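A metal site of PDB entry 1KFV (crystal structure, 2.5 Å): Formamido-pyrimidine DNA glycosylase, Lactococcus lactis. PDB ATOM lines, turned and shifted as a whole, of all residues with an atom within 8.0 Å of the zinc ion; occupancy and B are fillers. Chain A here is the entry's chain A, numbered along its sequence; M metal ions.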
ATOM      1  N   TRP A 179      -2.925  -0.478  15.996  1.00  0.00           N
ATOM      2  CA  TRP A 179      -2.398  -1.236  14.881  1.00  0.00           C
ATOM      3  C   TRP A 179      -2.554  -0.385  13.625  1.00  0.00           C
ATOM      4  O   TRP A 179      -1.600  -0.205  12.844  1.00  0.00           O
ATOM      5  CB  TRP A 179      -3.180  -2.533  14.700  1.00  0.00           C
ATOM      6  CG  TRP A 179      -2.782  -3.284  13.474  1.00  0.00           C
ATOM      7  CD1 TRP A 179      -1.757  -4.192  13.357  1.00  0.00           C
ATOM      8  CD2 TRP A 179      -3.395  -3.204  12.184  1.00  0.00           C
ATOM      9  NE1 TRP A 179      -1.701  -4.681  12.082  1.00  0.00           N
ATOM     10  CE2 TRP A 179      -2.698  -4.101  11.341  1.00  0.00           C
ATOM     11  CE3 TRP A 179      -4.472  -2.478  11.670  1.00  0.00           C
ATOM     12  CZ2 TRP A 179      -3.045  -4.272   9.996  1.00  0.00           C
ATOM     13  CZ3 TRP A 179      -4.808  -2.656  10.327  1.00  0.00           C
ATOM     14  CH2 TRP A 179      -4.107  -3.542   9.505  1.00  0.00           C
ATOM     15  N   LYS A 182       0.041   1.921  13.337  1.00  0.00           N
ATOM     16  CA  LYS A 182       1.377   1.342  13.420  1.00  0.00           C
ATOM     17  C   LYS A 182       2.165   1.743  14.672  1.00  0.00           C
ATOM     18  O   LYS A 182       3.387   1.862  14.633  1.00  0.00           O
ATOM     19  CB  LYS A 182       2.193   1.728  12.172  1.00  0.00           C
ATOM     20  CG  LYS A 182       1.709   1.061  10.875  1.00  0.00           C
ATOM     21  CD  LYS A 182       2.604   1.456   9.692  1.00  0.00           C
ATOM     22  CE  LYS A 182       2.177   0.772   8.394  1.00  0.00           C
ATOM     23  NZ  LYS A 182       3.142   1.037   7.265  1.00  0.00           N
ATOM     24  N   VAL A 237      -6.749  -7.087  14.432  1.00  0.00           N
ATOM     25  CA  VAL A 237      -5.824  -7.700  15.372  1.00  0.00           C
ATOM     26  C   VAL A 237      -6.393  -8.153  16.708  1.00  0.00           C
ATOM     27  O   VAL A 237      -5.808  -9.032  17.363  1.00  0.00           O
ATOM     28  CB  VAL A 237      -4.611  -6.769  15.680  1.00  0.00           C
ATOM     29  CG1 VAL A 237      -3.770  -6.546  14.425  1.00  0.00           C
ATOM     30  CG2 VAL A 237      -5.100  -5.428  16.247  1.00  0.00           C
ATOM     31  N   LYS A 244      -2.256 -14.073  10.508  1.00  0.00           N
ATOM     32  CA  LYS A 244      -1.365 -13.174   9.791  1.00  0.00           C
ATOM     33  C   LYS A 244      -1.856 -11.744   9.647  1.00  0.00           C
ATOM     34  O   LYS A 244      -3.048 -11.497   9.473  1.00  0.00           O
ATOM     35  CB  LYS A 244      -1.032 -13.773   8.417  1.00  0.00           C
ATOM     36  CG  LYS A 244      -0.196 -15.045   8.508  1.00  0.00           C
ATOM     37  CD  LYS A 244       0.245 -15.512   7.134  1.00  0.00           C
ATOM     38  CE  LYS A 244       1.301 -16.620   7.239  1.00  0.00           C
ATOM     39  NZ  LYS A 244       1.727 -17.128   5.908  1.00  0.00           N
ATOM     40  N   CYS A 245      -0.908 -10.807   9.744  1.00  0.00           N
ATOM     41  CA  CYS A 245      -1.173  -9.378   9.656  1.00  0.00           C
ATOM     42  C   CYS A 245      -1.643  -8.943   8.296  1.00  0.00           C
ATOM     43  O   CYS A 245      -0.972  -9.148   7.298  1.00  0.00           O
ATOM     44  CB  CYS A 245       0.064  -8.563  10.036  1.00  0.00           C
ATOM     45  SG  CYS A 245      -0.072  -6.806   9.616  1.00  0.00           S
ATOM     46  N   SER A 246      -2.803  -8.306   8.300  1.00  0.00           N
ATOM     47  CA  SER A 246      -3.457  -7.798   7.101  1.00  0.00           C
ATOM     48  C   SER A 246      -2.510  -7.179   6.103  1.00  0.00           C
ATOM     49  O   SER A 246      -2.701  -7.294   4.892  1.00  0.00           O
ATOM     50  CB  SER A 246      -4.514  -6.770   7.510  1.00  0.00           C
ATOM     51  OG  SER A 246      -5.027  -6.088   6.385  1.00  0.00           O
ATOM     52  N   ARG A 247      -1.470  -6.521   6.616  1.00  0.00           N
ATOM     53  CA  ARG A 247      -0.497  -5.853   5.755  1.00  0.00           C
ATOM     54  C   ARG A 247       0.817  -6.605   5.557  1.00  0.00           C
ATOM     55  O   ARG A 247       1.120  -7.011   4.436  1.00  0.00           O
ATOM     56  CB  ARG A 247      -0.218  -4.464   6.307  1.00  0.00           C
ATOM     57  CG  ARG A 247      -1.431  -3.547   6.315  1.00  0.00           C
ATOM     58  CD  ARG A 247      -1.114  -2.242   7.028  1.00  0.00           C
ATOM     59  NE  ARG A 247      -0.564  -2.490   8.362  1.00  0.00           N
ATOM     60  CZ  ARG A 247      -0.845  -1.755   9.437  1.00  0.00           C
ATOM     61  NH1 ARG A 247      -1.669  -0.726   9.362  1.00  0.00           N
ATOM     62  NH2 ARG A 247      -0.309  -2.082  10.605  1.00  0.00           N
ATOM     63  N   CYS A 248       1.599  -6.771   6.627  1.00  0.00           N
ATOM     64  CA  CYS A 248       2.897  -7.447   6.512  1.00  0.00           C
ATOM     65  C   CYS A 248       2.813  -8.974   6.593  1.00  0.00           C
ATOM     66  O   CYS A 248       3.791  -9.669   6.300  1.00  0.00           O
ATOM     67  CB  CYS A 248       3.879  -6.908   7.575  1.00  0.00           C
ATOM     68  SG  CYS A 248       3.838  -7.702   9.219  1.00  0.00           S
ATOM     69  N   GLY A 249       1.660  -9.491   6.990  1.00  0.00           N
ATOM     70  CA  GLY A 249       1.470 -10.934   7.067  1.00  0.00           C
ATOM     71  C   GLY A 249       2.044 -11.644   8.276  1.00  0.00           C
ATOM     72  O   GLY A 249       1.903 -12.858   8.418  1.00  0.00           O
ATOM     73  N   ALA A 250       2.696 -10.902   9.155  1.00  0.00           N
ATOM     74  CA  ALA A 250       3.296 -11.511  10.338  1.00  0.00           C
ATOM     75  C   ALA A 250       2.197 -12.026  11.274  1.00  0.00           C
ATOM     76  O   ALA A 250       1.047 -11.600  11.170  1.00  0.00           O
ATOM     77  CB  ALA A 250       4.179 -10.508  11.068  1.00  0.00           C
ATOM     78  N   GLU A 251       2.550 -12.944  12.160  1.00  0.00           N
ATOM     79  CA  GLU A 251       1.575 -13.502  13.098  1.00  0.00           C
ATOM     80  C   GLU A 251       1.243 -12.532  14.209  1.00  0.00           C
ATOM     81  O   GLU A 251       2.123 -12.105  14.956  1.00  0.00           O
ATOM     82  CB  GLU A 251       2.106 -14.798  13.716  1.00  0.00           C
ATOM     83  CG  GLU A 251       1.627 -16.048  13.016  1.00  0.00           C
ATOM     84  CD  GLU A 251       2.044 -17.311  13.729  1.00  0.00           C
ATOM     85  OE1 GLU A 251       1.589 -18.406  13.322  1.00  0.00           O
ATOM     86  OE2 GLU A 251       2.826 -17.207  14.701  1.00  0.00           O
ATOM     87  N   ILE A 252      -0.034 -12.183  14.324  1.00  0.00           N
ATOM     88  CA  ILE A 252      -0.466 -11.278  15.375  1.00  0.00           C
ATOM     89  C   ILE A 252      -0.106 -11.892  16.711  1.00  0.00           C
ATOM     90  O   ILE A 252      -0.392 -13.070  16.952  1.00  0.00           O
ATOM     91  CB  ILE A 252      -1.988 -11.047  15.347  1.00  0.00           C
ATOM     92  CG1 ILE A 252      -2.385 -10.442  13.995  1.00  0.00           C
ATOM     93  CG2 ILE A 252      -2.404 -10.157  16.503  1.00  0.00           C
ATOM     94  CD1 ILE A 252      -1.704  -9.112  13.687  1.00  0.00           C
ATOM     95  N   PHE A 264      -1.366  -7.071  18.779  1.00  0.00           N
ATOM     96  CA  PHE A 264      -0.640  -6.166  17.913  1.00  0.00           C
ATOM     97  C   PHE A 264       0.204  -6.950  16.926  1.00  0.00           C
ATOM     98  O   PHE A 264       0.239  -8.183  16.954  1.00  0.00           O
ATOM     99  CB  PHE A 264       0.270  -5.278  18.757  1.00  0.00           C
ATOM    100  CG  PHE A 264       1.433  -6.000  19.386  1.00  0.00           C
ATOM    101  CD1 PHE A 264       2.685  -5.994  18.787  1.00  0.00           C
ATOM    102  CD2 PHE A 264       1.262  -6.716  20.578  1.00  0.00           C
ATOM    103  CE1 PHE A 264       3.758  -6.686  19.359  1.00  0.00           C
ATOM    104  CE2 PHE A 264       2.330  -7.398  21.160  1.00  0.00           C
ATOM    105  CZ  PHE A 264       3.576  -7.380  20.547  1.00  0.00           C
ATOM    106  N   CYS A 265       0.888  -6.232  16.051  1.00  0.00           N
ATOM    107  CA  CYS A 265       1.762  -6.868  15.087  1.00  0.00           C
ATOM    108  C   CYS A 265       3.203  -6.487  15.389  1.00  0.00           C
ATOM    109  O   CYS A 265       3.547  -5.301  15.443  1.00  0.00           O
ATOM    110  CB  CYS A 265       1.437  -6.463  13.661  1.00  0.00           C
ATOM    111  SG  CYS A 265       2.585  -7.244  12.530  1.00  0.00           S
ATOM    112  N   PRO A 266       4.085  -7.490  15.567  1.00  0.00           N
ATOM    113  CA  PRO A 266       5.494  -7.281  15.869  1.00  0.00           C
ATOM    114  C   PRO A 266       6.177  -6.340  14.887  1.00  0.00           C
ATOM    115  O   PRO A 266       7.016  -5.535  15.287  1.00  0.00           O
ATOM    116  CB  PRO A 266       6.073  -8.681  15.802  1.00  0.00           C
ATOM    117  CG  PRO A 266       4.927  -9.525  16.234  1.00  0.00           C
ATOM    118  CD  PRO A 266       3.793  -8.929  15.462  1.00  0.00           C
ATOM    119  N   VAL A 267       5.801  -6.444  13.610  1.00  0.00           N
ATOM    120  CA  VAL A 267       6.404  -5.621  12.557  1.00  0.00           C
ATOM    121  C   VAL A 267       5.756  -4.264  12.264  1.00  0.00           C
ATOM    122  O   VAL A 267       6.449  -3.252  12.201  1.00  0.00           O
ATOM    123  CB  VAL A 267       6.476  -6.402  11.243  1.00  0.00           C
ATOM    124  CG1 VAL A 267       7.327  -5.641  10.240  1.00  0.00           C
ATOM    125  CG2 VAL A 267       7.047  -7.788  11.480  1.00  0.00           C
ATOM    126  N   CYS A 268       4.437  -4.243  12.051  1.00  0.00           N
ATOM    127  CA  CYS A 268       3.759  -2.981  11.779  1.00  0.00           C
ATOM    128  C   CYS A 268       3.805  -2.059  12.971  1.00  0.00           C
ATOM    129  O   CYS A 268       3.900  -0.848  12.835  1.00  0.00           O
ATOM    130  CB  CYS A 268       2.303  -3.216  11.409  1.00  0.00           C
ATOM    131  SG  CYS A 268       2.090  -3.959   9.824  1.00  0.00           S
ATOM    132  N   GLN A 269       3.735  -2.659  14.154  1.00  0.00           N
ATOM    133  CA  GLN A 269       3.771  -1.899  15.399  1.00  0.00           C
ATOM    134  C   GLN A 269       5.170  -2.056  15.986  1.00  0.00           C
ATOM    135  O   GLN A 269       5.417  -2.928  16.823  1.00  0.00           O
ATOM    136  CB  GLN A 269       2.676  -2.423  16.326  1.00  0.00           C
ATOM    137  CG  GLN A 269       1.269  -2.137  15.764  1.00  0.00           C
ATOM    138  CD  GLN A 269       0.173  -2.955  16.399  1.00  0.00           C
ATOM    139  OE1 GLN A 269      -0.214  -3.999  15.877  1.00  0.00           O
ATOM    140  NE2 GLN A 269      -0.328  -2.500  17.532  1.00  0.00           N
HETATM  141 ZN    ZN M   1       2.053  -6.174  10.259  1.00  0.00          ZN
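Of the 18 residues printed, 4 come within 4 Å of the zinc ion. The nearest printed residue that does not touch the zinc ion is Trp 179 (4.4 Å).
The zinc ion is bound by the side-chain sulfur of Cys 268 (2.3 Å), the side-chain sulfur of Cys 245 (2.3 Å), the side-chain sulfur of Cys 265 (2.6 Å) and the side-chain sulfur of Cys 248 (2.6 Å).
The backbone NH (N) of Cys 245 is in hydrogen-bond range of the backbone carbonyl oxygen (O) of Ala 250 (2.5 Å). NH2 of Arg 247 sits close to SG of Cys 268 (3.1 Å). The backbone NH of Cys 265 sits at hydrogen-bond distance from the side-chain amide oxygen of Gln 269, at 2.5 Å. NE1 of Trp 179 lies close to SG of Cys 245, at 3.6 Å. The backbone NH (N) of Ala 250 lies close to the side-chain sulfur (SG) of Cys 248 (3.4 Å). The backbone NH (N) of Arg 247 lies close to the side-chain sulfur (SG) of Cys 245. The side-chain sulfur (SG) of Cys 265 lies close to the backbone NH (N) of Val 267 (3.5 Å).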
